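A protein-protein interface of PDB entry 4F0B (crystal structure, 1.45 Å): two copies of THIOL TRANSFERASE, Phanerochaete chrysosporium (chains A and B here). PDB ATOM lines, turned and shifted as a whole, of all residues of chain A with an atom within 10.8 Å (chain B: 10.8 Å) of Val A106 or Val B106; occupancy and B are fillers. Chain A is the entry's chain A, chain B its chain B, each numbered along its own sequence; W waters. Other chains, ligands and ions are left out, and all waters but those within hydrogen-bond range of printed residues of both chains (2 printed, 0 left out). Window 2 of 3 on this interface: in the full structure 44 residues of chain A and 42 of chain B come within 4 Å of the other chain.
Gln A93 touches Pro B105, and with the chains exchanged Pro A105 touches Gln B93.
Gln A93 touches Pro B109, and with the chains exchanged Pro A109 touches Gln B93.
His A94 touches Lys B110, but with the chains exchanged Lys A110 does not touch His B94 (5.7 Å).
Val B106 touches its own counterpart, Val A106.
Positions printed for both chains: 93, 94, 97, 99, 102, 103, 104, 105, 106, 107, 108, 109, 110, 111, 112, 113, 115 and 116.
Of the 7 pairs that touch across the chains among the printed residues, 6 have their exchanged pair printed and touching as well.
Water W1 lies within hydrogen-bond range of NE2 of His A94 and NZ of Lys B110.
Water W2 lies within hydrogen-bond range of O of Pro A109 (2.7 Å) and OE1 of Gln B93 (2.9 Å).
Of the 18 printed residues of chain B, 6 touch a printed residue of chain A.
Printed residues of chain B that touch a printed residue of chain A: Gln B93, Pro B105, Val B106, Pro B109, Lys B110 and Tyr B112.
Hydrophobic or aromatic side chains of chain B that line the printed part of chain A: Val B106, Pro B109 and Tyr B112.
Hydrophobic or aromatic side chains of chain A within 4 Å of the printed part of chain B: His A94, Val A106, Pro A109 and Tyr A112.
Among the printed residues, pairs that only touch across the chains: Val A106 with Val B106, Pro A109 with Gln B93, Gln A93 with Pro B109 and His A94 with Lys B110.
The side-chain carboxylate (OD2) of Asp B104 lies within hydrogen-bond range of the backbone NH (N) of Val B106, 2.9 Å away.
The backbone carbonyl oxygen of Gln B93 is in hydrogen-bond range of the side-chain amino group of Lys B97.
The side-chain carboxylate (OD2) of Asp A104 lies within hydrogen-bond range of the backbone NH (N) of Val A106, at 2.9 Å.
O of Gln A93 lies within hydrogen-bond range of NZ of Lys A97 (3.0 Å).
The side-chain amide nitrogen (NE2) of Gln B93 lies close to a ring nitrogen (ND1) of His B94 (3.5 Å).
O of Pro A105 sits close to OE1 of Gln B93 (3.4 Å).
OH of Tyr A112 sits at hydrogen-bond distance from OH of Tyr B112, 2.7 Å away.
The backbone carbonyl oxygen (O) of Pro B105 sits at hydrogen-bond distance from the side-chain amide nitrogen (NE2) of Gln A93 (2.8 Å).
Of the printed residues of chain B, Gln A93 touches Pro B105 (2.8 Å) and Pro B109 (3.8 Å).
No residue of chain B comes within 4 Å of Asp A104.
Val A106 touches just one residue of chain B: Val B106 (3.5 Å).
Of the printed residues of chain B, Pro A109 touches Gln B93.
Asn B99 touches none of the printed residues of chain A.
No residue of chain A comes within 4 Å of Asp B104.
Of chain A, only Gln A93 comes within 4 Å of Pro B105.
Of chain A, only Val A106 comes within 4 Å of Val B106.
Of the printed residues of chain A, Lys B110 touches His A94.
The nearest printed residue of chain B that does not touch Val A106 is Gln B93 (5.4 Å).
The nearest residue of chain A that does not touch Val B106 is Gln A93 (4.7 Å).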
ATOM      1  N   GLN A  93     -10.276  -8.479   0.238  1.00  0.00           N
ATOM      2  CA  GLN A  93     -10.762  -7.182   0.685  1.00  0.00           C
ATOM      3  C   GLN A  93      -9.877  -6.048   0.166  1.00  0.00           C
ATOM      4  O   GLN A  93     -10.368  -4.984  -0.193  1.00  0.00           O
ATOM      5  CB  GLN A  93     -10.857  -7.140   2.225  1.00  0.00           C
ATOM      6  CG  GLN A  93     -11.212  -5.729   2.777  1.00  0.00           C
ATOM      7  CD  GLN A  93     -11.379  -5.692   4.310  1.00  0.00           C
ATOM      8  OE1 GLN A  93     -10.966  -6.613   5.005  1.00  0.00           O
ATOM      9  NE2 GLN A  93     -12.011  -4.637   4.823  1.00  0.00           N
ATOM     10  N   HIS A  94      -8.581  -6.316   0.107  1.00  0.00           N
ATOM     11  CA  HIS A  94      -7.595  -5.304  -0.239  1.00  0.00           C
ATOM     12  C   HIS A  94      -7.313  -5.159  -1.736  1.00  0.00           C
ATOM     13  O   HIS A  94      -6.936  -4.075  -2.190  1.00  0.00           O
ATOM     14  CB  HIS A  94      -6.329  -5.556   0.565  1.00  0.00           C
ATOM     15  CG  HIS A  94      -6.471  -5.148   1.993  1.00  0.00           C
ATOM     16  ND1 HIS A  94      -7.129  -5.921   2.936  1.00  0.00           N
ATOM     17  CD2 HIS A  94      -6.116  -4.001   2.617  1.00  0.00           C
ATOM     18  CE1 HIS A  94      -7.149  -5.266   4.085  1.00  0.00           C
ATOM     19  NE2 HIS A  94      -6.525  -4.109   3.923  1.00  0.00           N
ATOM     20  N   LYS A  97     -11.109  -5.410  -6.000  1.00  0.00           N
ATOM     21  CA  LYS A  97     -11.967  -4.227  -5.939  1.00  0.00           C
ATOM     22  C   LYS A  97     -13.273  -4.338  -6.718  1.00  0.00           C
ATOM     23  O   LYS A  97     -14.247  -3.651  -6.403  1.00  0.00           O
ATOM     24  CB  LYS A  97     -11.181  -2.974  -6.352  1.00  0.00           C
ATOM     25  CG  LYS A  97     -10.200  -2.523  -5.253  1.00  0.00           C
ATOM     26  CD  LYS A  97     -10.869  -2.560  -3.867  1.00  0.00           C
ATOM     27  CE  LYS A  97      -9.887  -2.200  -2.752  1.00  0.00           C
ATOM     28  NZ  LYS A  97     -10.524  -2.242  -1.392  1.00  0.00           N
ATOM     29  N   ASN A  99     -14.796  -7.354  -6.961  1.00  0.00           N
ATOM     30  CA  ASN A  99     -15.462  -8.557  -6.453  1.00  0.00           C
ATOM     31  C   ASN A  99     -15.603  -9.650  -7.520  1.00  0.00           C
ATOM     32  O   ASN A  99     -16.673 -10.229  -7.745  1.00  0.00           O
ATOM     33  CB  ASN A  99     -16.807  -8.173  -5.820  1.00  0.00           C
ATOM     34  CG  ASN A  99     -16.628  -7.402  -4.520  1.00  0.00           C
ATOM     35  OD1 ASN A  99     -16.928  -6.209  -4.445  1.00  0.00           O
ATOM     36  ND2 ASN A  99     -16.108  -8.068  -3.508  1.00  0.00           N
ATOM     37  N   SER A 102     -14.886 -12.779  -4.808  1.00  0.00           N
ATOM     38  CA  SER A 102     -15.257 -12.635  -3.405  1.00  0.00           C
ATOM     39  C   SER A 102     -16.465 -11.742  -3.300  1.00  0.00           C
ATOM     40  O   SER A 102     -16.752 -10.972  -4.220  1.00  0.00           O
ATOM     41  CB  SER A 102     -14.102 -11.991  -2.621  1.00  0.00           C
ATOM     42  OG  SER A 102     -13.841 -10.655  -3.100  1.00  0.00           O
ATOM     43  N   ARG A 103     -17.189 -11.817  -2.191  1.00  0.00           N
ATOM     44  CA  ARG A 103     -18.367 -10.977  -2.012  1.00  0.00           C
ATOM     45  C   ARG A 103     -18.060  -9.871  -0.996  1.00  0.00           C
ATOM     46  O   ARG A 103     -17.283 -10.084  -0.076  1.00  0.00           O
ATOM     47  CB  ARG A 103     -19.552 -11.829  -1.533  1.00  0.00           C
ATOM     48  CG  ARG A 103     -19.756 -13.157  -2.260  1.00  0.00           C
ATOM     49  CD  ARG A 103     -19.639 -13.028  -3.750  1.00  0.00           C
ATOM     50  NE  ARG A 103     -19.919 -14.288  -4.450  1.00  0.00           N
ATOM     51  CZ  ARG A 103     -19.015 -15.236  -4.710  1.00  0.00           C
ATOM     52  NH1 ARG A 103     -17.748 -15.090  -4.345  1.00  0.00           N
ATOM     53  NH2 ARG A 103     -19.370 -16.315  -5.377  1.00  0.00           N
ATOM     54  N   ASP A 104     -18.652  -8.685  -1.180  1.00  0.00           N
ATOM     55  CA  ASP A 104     -18.424  -7.539  -0.315  1.00  0.00           C
ATOM     56  C   ASP A 104     -19.336  -7.569   0.924  1.00  0.00           C
ATOM     57  O   ASP A 104     -20.545  -7.718   0.796  1.00  0.00           O
ATOM     58  CB  ASP A 104     -18.653  -6.252  -1.089  1.00  0.00           C
ATOM     59  CG  ASP A 104     -18.292  -5.070  -0.268  1.00  0.00           C
ATOM     60  OD1 ASP A 104     -17.082  -4.781  -0.204  1.00  0.00           O
ATOM     61  OD2 ASP A 104     -19.199  -4.508   0.365  1.00  0.00           O
ATOM     62  N   PRO A 105     -18.757  -7.382   2.123  1.00  0.00           N
ATOM     63  CA  PRO A 105     -19.574  -7.498   3.340  1.00  0.00           C
ATOM     64  C   PRO A 105     -20.645  -6.426   3.479  1.00  0.00           C
ATOM     65  O   PRO A 105     -21.674  -6.673   4.117  1.00  0.00           O
ATOM     66  CB  PRO A 105     -18.547  -7.379   4.479  1.00  0.00           C
ATOM     67  CG  PRO A 105     -17.309  -6.785   3.859  1.00  0.00           C
ATOM     68  CD  PRO A 105     -17.317  -7.227   2.414  1.00  0.00           C
ATOM     69  N   VAL A 106     -20.420  -5.252   2.892  1.00  0.00           N
ATOM     70  CA  VAL A 106     -21.365  -4.158   3.027  1.00  0.00           C
ATOM     71  C   VAL A 106     -22.451  -4.261   1.978  1.00  0.00           C
ATOM     72  O   VAL A 106     -23.631  -4.158   2.292  1.00  0.00           O
ATOM     73  CB  VAL A 106     -20.644  -2.808   2.910  1.00  0.00           C
ATOM     74  CG1 VAL A 106     -21.630  -1.653   2.812  1.00  0.00           C
ATOM     75  CG2 VAL A 106     -19.710  -2.636   4.102  1.00  0.00           C
ATOM     76  N   LYS A 107     -22.053  -4.479   0.737  1.00  0.00           N
ATOM     77  CA  LYS A 107     -23.032  -4.493  -0.354  1.00  0.00           C
ATOM     78  C   LYS A 107     -23.796  -5.805  -0.448  1.00  0.00           C
ATOM     79  O   LYS A 107     -24.908  -5.834  -0.997  1.00  0.00           O
ATOM     80  CB  LYS A 107     -22.332  -4.253  -1.690  1.00  0.00           C
ATOM     81  CG  LYS A 107     -21.587  -2.919  -1.767  1.00  0.00           C
ATOM     82  CD  LYS A 107     -20.703  -2.873  -3.009  1.00  0.00           C
ATOM     83  CE  LYS A 107     -20.041  -1.508  -3.183  1.00  0.00           C
ATOM     84  NZ  LYS A 107     -18.553  -1.636  -3.084  1.00  0.00           N
ATOM     85  N   ASP A 108     -23.209  -6.891   0.062  1.00  0.00           N
ATOM     86  CA  ASP A 108     -23.824  -8.198  -0.076  1.00  0.00           C
ATOM     87  C   ASP A 108     -23.638  -8.956   1.243  1.00  0.00           C
ATOM     88  O   ASP A 108     -22.928  -9.951   1.296  1.00  0.00           O
ATOM     89  CB  ASP A 108     -23.141  -8.955  -1.216  1.00  0.00           C
ATOM     90  CG  ASP A 108     -23.792 -10.281  -1.541  1.00  0.00           C
ATOM     91  OD1 ASP A 108     -24.886 -10.592  -1.023  1.00  0.00           O
ATOM     92  OD2 ASP A 108     -23.181 -11.012  -2.352  1.00  0.00           O
ATOM     93  N   PRO A 109     -24.285  -8.495   2.318  1.00  0.00           N
ATOM     94  CA  PRO A 109     -24.103  -9.200   3.600  1.00  0.00           C
ATOM     95  C   PRO A 109     -24.522 -10.674   3.575  1.00  0.00           C
ATOM     96  O   PRO A 109     -23.851 -11.504   4.219  1.00  0.00           O
ATOM     97  CB  PRO A 109     -24.979  -8.411   4.581  1.00  0.00           C
ATOM     98  CG  PRO A 109     -25.884  -7.568   3.726  1.00  0.00           C
ATOM     99  CD  PRO A 109     -25.219  -7.358   2.412  1.00  0.00           C
ATOM    100  N   LYS A 110     -25.571 -11.031   2.845  1.00  0.00           N
ATOM    101  CA  LYS A 110     -25.948 -12.449   2.784  1.00  0.00           C
ATOM    102  C   LYS A 110     -24.922 -13.287   2.030  1.00  0.00           C
ATOM    103  O   LYS A 110     -24.535 -14.351   2.486  1.00  0.00           O
ATOM    104  CB  LYS A 110     -27.338 -12.647   2.178  1.00  0.00           C
ATOM    105  CG  LYS A 110     -28.465 -12.101   3.023  1.00  0.00           C
ATOM    106  CD  LYS A 110     -29.806 -12.426   2.386  1.00  0.00           C
ATOM    107  CE  LYS A 110     -30.937 -12.173   3.350  1.00  0.00           C
ATOM    108  NZ  LYS A 110     -32.265 -12.329   2.650  1.00  0.00           N
ATOM    109  N   GLY A 111     -24.470 -12.807   0.877  1.00  0.00           N
ATOM    110  CA  GLY A 111     -23.507 -13.549   0.111  1.00  0.00           C
ATOM    111  C   GLY A 111     -22.163 -13.637   0.805  1.00  0.00           C
ATOM    112  O   GLY A 111     -21.485 -14.652   0.765  1.00  0.00           O
ATOM    113  N   TYR A 112     -21.774 -12.545   1.470  1.00  0.00           N
ATOM    114  CA  TYR A 112     -20.555 -12.547   2.261  1.00  0.00           C
ATOM    115  C   TYR A 112     -20.668 -13.564   3.392  1.00  0.00           C
ATOM    116  O   TYR A 112     -19.740 -14.339   3.632  1.00  0.00           O
ATOM    117  CB  TYR A 112     -20.266 -11.137   2.811  1.00  0.00           C
ATOM    118  CG  TYR A 112     -19.008 -11.063   3.640  1.00  0.00           C
ATOM    119  CD1 TYR A 112     -17.756 -11.119   3.021  1.00  0.00           C
ATOM    120  CD2 TYR A 112     -19.062 -10.940   5.022  1.00  0.00           C
ATOM    121  CE1 TYR A 112     -16.573 -11.049   3.771  1.00  0.00           C
ATOM    122  CE2 TYR A 112     -17.891 -10.887   5.786  1.00  0.00           C
ATOM    123  CZ  TYR A 112     -16.666 -10.933   5.146  1.00  0.00           C
ATOM    124  OH  TYR A 112     -15.491 -10.878   5.897  1.00  0.00           O
ATOM    125  N   SER A 113     -21.805 -13.586   4.090  1.00  0.00           N
ATOM    126  CA  SER A 113     -21.990 -14.617   5.109  1.00  0.00           C
ATOM    127  C   SER A 113     -21.886 -16.030   4.536  1.00  0.00           C
ATOM    128  O   SER A 113     -21.216 -16.876   5.100  1.00  0.00           O
ATOM    129  CB  SER A 113     -23.322 -14.431   5.808  1.00  0.00           C
ATOM    130  OG  SER A 113     -23.497 -15.494   6.759  1.00  0.00           O
ATOM    131  N   GLU A 115     -20.216 -17.009   1.947  1.00  0.00           N
ATOM    132  CA  GLU A 115     -18.814 -17.242   1.691  1.00  0.00           C
ATOM    133  C   GLU A 115     -18.064 -17.599   2.986  1.00  0.00           C
ATOM    134  O   GLU A 115     -17.288 -18.562   2.993  1.00  0.00           O
ATOM    135  CB  GLU A 115     -18.247 -16.003   0.998  1.00  0.00           C
ATOM    136  CG  GLU A 115     -16.772 -16.082   0.721  1.00  0.00           C
ATOM    137  CD  GLU A 115     -16.259 -14.746   0.345  1.00  0.00           C
ATOM    138  OE1 GLU A 115     -15.836 -13.995   1.257  1.00  0.00           O
ATOM    139  OE2 GLU A 115     -16.366 -14.394  -0.840  1.00  0.00           O
ATOM    140  N   LEU A 116     -18.283 -16.848   4.065  1.00  0.00           N
ATOM    141  CA  LEU A 116     -17.682 -17.191   5.364  1.00  0.00           C
ATOM    142  C   LEU A 116     -18.103 -18.582   5.828  1.00  0.00           C
ATOM    143  O   LEU A 116     -17.289 -19.358   6.318  1.00  0.00           O
ATOM    144  CB  LEU A 116     -18.072 -16.190   6.453  1.00  0.00           C
ATOM    145  CG  LEU A 116     -17.506 -14.778   6.324  1.00  0.00           C
ATOM    146  CD1 LEU A 116     -18.019 -13.943   7.482  1.00  0.00           C
ATOM    147  CD2 LEU A 116     -15.967 -14.822   6.340  1.00  0.00           C
ATOM    148  N   GLN B  93     -22.269  -8.627  12.811  1.00  0.00           N
ATOM    149  CA  GLN B  93     -22.411  -7.613  11.764  1.00  0.00           C
ATOM    150  C   GLN B  93     -23.850  -7.048  11.775  1.00  0.00           C
ATOM    151  O   GLN B  93     -24.055  -5.859  11.523  1.00  0.00           O
ATOM    152  CB  GLN B  93     -22.090  -8.247  10.410  1.00  0.00           C
ATOM    153  CG  GLN B  93     -21.991  -7.277   9.242  1.00  0.00           C
ATOM    154  CD  GLN B  93     -22.631  -7.796   7.959  1.00  0.00           C
ATOM    155  OE1 GLN B  93     -21.949  -8.308   7.037  1.00  0.00           O
ATOM    156  NE2 GLN B  93     -23.953  -7.627   7.872  1.00  0.00           N
ATOM    157  N   HIS B  94     -24.827  -7.920  12.074  1.00  0.00           N
ATOM    158  CA  HIS B  94     -26.250  -7.530  12.051  1.00  0.00           C
ATOM    159  C   HIS B  94     -26.799  -6.885  13.325  1.00  0.00           C
ATOM    160  O   HIS B  94     -27.802  -6.167  13.267  1.00  0.00           O
ATOM    161  CB  HIS B  94     -27.113  -8.766  11.697  1.00  0.00           C
ATOM    162  CG  HIS B  94     -26.986  -9.182  10.268  1.00  0.00           C
ATOM    163  ND1 HIS B  94     -25.873  -9.829   9.773  1.00  0.00           N
ATOM    164  CD2 HIS B  94     -27.797  -8.963   9.203  1.00  0.00           C
ATOM    165  CE1 HIS B  94     -26.011 -10.003   8.469  1.00  0.00           C
ATOM    166  NE2 HIS B  94     -27.177  -9.504   8.103  1.00  0.00           N
ATOM    167  N   LYS B  97     -24.073  -2.980  16.511  1.00  0.00           N
ATOM    168  CA  LYS B  97     -23.892  -1.730  15.779  1.00  0.00           C
ATOM    169  C   LYS B  97     -22.873  -0.787  16.369  1.00  0.00           C
ATOM    170  O   LYS B  97     -22.375   0.102  15.668  1.00  0.00           O
ATOM    171  CB  LYS B  97     -25.232  -1.015  15.586  1.00  0.00           C
ATOM    172  CG  LYS B  97     -26.229  -1.789  14.700  1.00  0.00           C
ATOM    173  CD  LYS B  97     -25.556  -2.358  13.445  1.00  0.00           C
ATOM    174  CE  LYS B  97     -26.569  -2.653  12.324  1.00  0.00           C
ATOM    175  NZ  LYS B  97     -25.914  -3.348  11.150  1.00  0.00           N
ATOM    176  N   ASN B  99     -20.105  -1.972  17.823  1.00  0.00           N
ATOM    177  CA  ASN B  99     -18.846  -2.704  17.911  1.00  0.00           C
ATOM    178  C   ASN B  99     -18.367  -2.958  19.335  1.00  0.00           C
ATOM    179  O   ASN B  99     -17.187  -2.737  19.695  1.00  0.00           O
ATOM    180  CB  ASN B  99     -17.763  -2.016  17.055  1.00  0.00           C
ATOM    181  CG  ASN B  99     -18.129  -1.999  15.570  1.00  0.00           C
ATOM    182  OD1 ASN B  99     -18.555  -0.954  15.048  1.00  0.00           O
ATOM    183  ND2 ASN B  99     -17.980  -3.134  14.896  1.00  0.00           N
ATOM    184  N   SER B 102     -17.003  -6.853  18.468  1.00  0.00           N
ATOM    185  CA  SER B 102     -16.519  -7.203  17.137  1.00  0.00           C
ATOM    186  C   SER B 102     -15.933  -5.946  16.498  1.00  0.00           C
ATOM    187  O   SER B 102     -16.259  -4.813  16.900  1.00  0.00           O
ATOM    188  CB  SER B 102     -17.643  -7.716  16.294  1.00  0.00           C
ATOM    189  OG  SER B 102     -18.593  -6.656  16.126  1.00  0.00           O
ATOM    190  N   ARG B 103     -15.067  -6.171  15.520  1.00  0.00           N
ATOM    191  CA  ARG B 103     -14.443  -5.064  14.797  1.00  0.00           C
ATOM    192  C   ARG B 103     -15.109  -4.827  13.446  1.00  0.00           C
ATOM    193  O   ARG B 103     -15.625  -5.751  12.805  1.00  0.00           O
ATOM    194  CB  ARG B 103     -12.955  -5.317  14.643  1.00  0.00           C
ATOM    195  CG  ARG B 103     -12.231  -5.279  15.988  1.00  0.00           C
ATOM    196  CD  ARG B 103     -10.854  -5.755  15.880  1.00  0.00           C
ATOM    197  NE  ARG B 103     -10.111  -5.496  17.107  1.00  0.00           N
ATOM    198  CZ  ARG B 103      -8.839  -5.830  17.265  1.00  0.00           C
ATOM    199  NH1 ARG B 103      -8.193  -6.455  16.291  1.00  0.00           N
ATOM    200  NH2 ARG B 103      -8.220  -5.529  18.415  1.00  0.00           N
ATOM    201  N   ASP B 104     -15.130  -3.576  13.019  1.00  0.00           N
ATOM    202  CA  ASP B 104     -15.794  -3.240  11.759  1.00  0.00           C
ATOM    203  C   ASP B 104     -14.863  -3.411  10.547  1.00  0.00           C
ATOM    204  O   ASP B 104     -13.761  -2.878  10.518  1.00  0.00           O
ATOM    205  CB  ASP B 104     -16.321  -1.811  11.792  1.00  0.00           C
ATOM    206  CG  ASP B 104     -17.121  -1.503  10.549  1.00  0.00           C
ATOM    207  OD1 ASP B 104     -18.283  -1.965  10.475  1.00  0.00           O
ATOM    208  OD2 ASP B 104     -16.566  -0.892   9.635  1.00  0.00           O
ATOM    209  N   PRO B 105     -15.314  -4.160   9.537  1.00  0.00           N
ATOM    210  CA  PRO B 105     -14.440  -4.416   8.385  1.00  0.00           C
ATOM    211  C   PRO B 105     -14.068  -3.163   7.600  1.00  0.00           C
ATOM    212  O   PRO B 105     -13.001  -3.140   6.986  1.00  0.00           O
ATOM    213  CB  PRO B 105     -15.293  -5.331   7.477  1.00  0.00           C
ATOM    214  CG  PRO B 105     -16.406  -5.805   8.304  1.00  0.00           C
ATOM    215  CD  PRO B 105     -16.589  -4.900   9.474  1.00  0.00           C
ATOM    216  N   VAL B 106     -14.937  -2.148   7.573  1.00  0.00           N
ATOM    217  CA  VAL B 106     -14.695  -0.951   6.747  1.00  0.00           C
ATOM    218  C   VAL B 106     -13.789   0.044   7.454  1.00  0.00           C
ATOM    219  O   VAL B 106     -12.784   0.494   6.891  1.00  0.00           O
ATOM    220  CB  VAL B 106     -16.021  -0.270   6.412  1.00  0.00           C
ATOM    221  CG1 VAL B 106     -15.774   1.076   5.714  1.00  0.00           C
ATOM    222  CG2 VAL B 106     -16.857  -1.199   5.548  1.00  0.00           C
ATOM    223  N   LYS B 107     -14.125   0.341   8.708  1.00  0.00           N
ATOM    224  CA  LYS B 107     -13.401   1.355   9.473  1.00  0.00           C
ATOM    225  C   LYS B 107     -12.153   0.818  10.169  1.00  0.00           C
ATOM    226  O   LYS B 107     -11.280   1.593  10.565  1.00  0.00           O
ATOM    227  CB  LYS B 107     -14.332   1.957  10.527  1.00  0.00           C
ATOM    228  CG  LYS B 107     -15.489   2.711   9.917  1.00  0.00           C
ATOM    229  CD  LYS B 107     -16.232   3.507  10.973  1.00  0.00           C
ATOM    230  CE  LYS B 107     -17.195   4.491  10.336  1.00  0.00           C
ATOM    231  NZ  LYS B 107     -17.529   5.605  11.275  1.00  0.00           N
ATOM    232  N   ASP B 108     -12.081  -0.505  10.338  1.00  0.00           N
ATOM    233  CA  ASP B 108     -10.921  -1.133  10.988  1.00  0.00           C
ATOM    234  C   ASP B 108     -10.524  -2.395  10.207  1.00  0.00           C
ATOM    235  O   ASP B 108     -10.590  -3.507  10.753  1.00  0.00           O
ATOM    236  CB  ASP B 108     -11.251  -1.455  12.446  1.00  0.00           C
ATOM    237  CG  ASP B 108     -10.054  -1.976  13.253  1.00  0.00           C
ATOM    238  OD1 ASP B 108      -8.904  -1.875  12.821  1.00  0.00           O
ATOM    239  OD2 ASP B 108     -10.299  -2.454  14.372  1.00  0.00           O
ATOM    240  N   PRO B 109     -10.086  -2.239   8.953  1.00  0.00           N
ATOM    241  CA  PRO B 109      -9.759  -3.432   8.151  1.00  0.00           C
ATOM    242  C   PRO B 109      -8.639  -4.290   8.780  1.00  0.00           C
ATOM    243  O   PRO B 109      -8.673  -5.520   8.733  1.00  0.00           O
ATOM    244  CB  PRO B 109      -9.308  -2.864   6.793  1.00  0.00           C
ATOM    245  CG  PRO B 109      -9.117  -1.376   7.050  1.00  0.00           C
ATOM    246  CD  PRO B 109     -10.024  -0.991   8.158  1.00  0.00           C
ATOM    247  N   LYS B 110      -7.641  -3.639   9.368  1.00  0.00           N
ATOM    248  CA  LYS B 110      -6.573  -4.415   9.984  1.00  0.00           C
ATOM    249  C   LYS B 110      -7.047  -5.126  11.241  1.00  0.00           C
ATOM    250  O   LYS B 110      -6.746  -6.320  11.442  1.00  0.00           O
ATOM    251  CB  LYS B 110      -5.375  -3.524  10.329  1.00  0.00           C
ATOM    252  CG  LYS B 110      -4.792  -2.712   9.171  1.00  0.00           C
ATOM    253  CD  LYS B 110      -4.429  -3.595   8.010  1.00  0.00           C
ATOM    254  CE  LYS B 110      -3.343  -2.908   7.199  1.00  0.00           C
ATOM    255  NZ  LYS B 110      -3.251  -3.255   5.782  1.00  0.00           N
ATOM    256  N   GLY B 111      -7.799  -4.446  12.105  1.00  0.00           N
ATOM    257  CA  GLY B 111      -8.314  -5.083  13.295  1.00  0.00           C
ATOM    258  C   GLY B 111      -9.297  -6.203  12.962  1.00  0.00           C
ATOM    259  O   GLY B 111      -9.301  -7.256  13.617  1.00  0.00           O
ATOM    260  N   TYR B 112     -10.140  -5.982  11.954  1.00  0.00           N
ATOM    261  CA  TYR B 112     -11.066  -7.013  11.508  1.00  0.00           C
ATOM    262  C   TYR B 112     -10.295  -8.239  11.014  1.00  0.00           C
ATOM    263  O   TYR B 112     -10.674  -9.377  11.318  1.00  0.00           O
ATOM    264  CB  TYR B 112     -11.993  -6.436  10.426  1.00  0.00           C
ATOM    265  CG  TYR B 112     -12.973  -7.434   9.886  1.00  0.00           C
ATOM    266  CD1 TYR B 112     -13.986  -7.933  10.703  1.00  0.00           C
ATOM    267  CD2 TYR B 112     -12.858  -7.919   8.587  1.00  0.00           C
ATOM    268  CE1 TYR B 112     -14.892  -8.882  10.228  1.00  0.00           C
ATOM    269  CE2 TYR B 112     -13.762  -8.873   8.098  1.00  0.00           C
ATOM    270  CZ  TYR B 112     -14.766  -9.331   8.930  1.00  0.00           C
ATOM    271  OH  TYR B 112     -15.692 -10.289   8.498  1.00  0.00           O
ATOM    272  N   SER B 113      -9.239  -8.006  10.226  1.00  0.00           N
ATOM    273  CA  SER B 113      -8.407  -9.122   9.787  1.00  0.00           C
ATOM    274  C   SER B 113      -7.837  -9.884  10.975  1.00  0.00           C
ATOM    275  O   SER B 113      -7.879 -11.114  10.982  1.00  0.00           O
ATOM    276  CB  SER B 113      -7.281  -8.672   8.874  1.00  0.00           C
ATOM    277  OG  SER B 113      -6.507  -9.806   8.509  1.00  0.00           O
ATOM    278  N   GLU B 115      -9.102 -10.217  13.918  1.00  0.00           N
ATOM    279  CA  GLU B 115     -10.217 -10.984  14.481  1.00  0.00           C
ATOM    280  C   GLU B 115     -10.469 -12.238  13.667  1.00  0.00           C
ATOM    281  O   GLU B 115     -10.613 -13.340  14.242  1.00  0.00           O
ATOM    282  CB  GLU B 115     -11.434 -10.075  14.527  1.00  0.00           C
ATOM    283  CG  GLU B 115     -12.645 -10.687  15.176  1.00  0.00           C
ATOM    284  CD  GLU B 115     -13.846  -9.815  14.865  1.00  0.00           C
ATOM    285  OE1 GLU B 115     -14.071  -8.834  15.569  1.00  0.00           O
ATOM    286  OE2 GLU B 115     -14.529 -10.058  13.843  1.00  0.00           O
ATOM    287  N   LEU B 116     -10.496 -12.116  12.339  1.00  0.00           N
ATOM    288  CA  LEU B 116     -10.664 -13.291  11.497  1.00  0.00           C
ATOM    289  C   LEU B 116      -9.530 -14.299  11.693  1.00  0.00           C
ATOM    290  O   LEU B 116      -9.769 -15.524  11.749  1.00  0.00           O
ATOM    291  CB  LEU B 116     -10.737 -12.903  10.015  1.00  0.00           C
ATOM    292  CG  LEU B 116     -12.010 -12.164   9.591  1.00  0.00           C
ATOM    293  CD1 LEU B 116     -11.882 -11.806   8.092  1.00  0.00           C
ATOM    294  CD2 LEU B 116     -13.268 -13.012   9.787  1.00  0.00           C
HETATM  295  O   HOH W   1      -5.935  -1.944   5.300  1.00  0.00           O
HETATM  296  O   HOH W   2     -23.241 -10.844   6.794  1.00  0.00           O
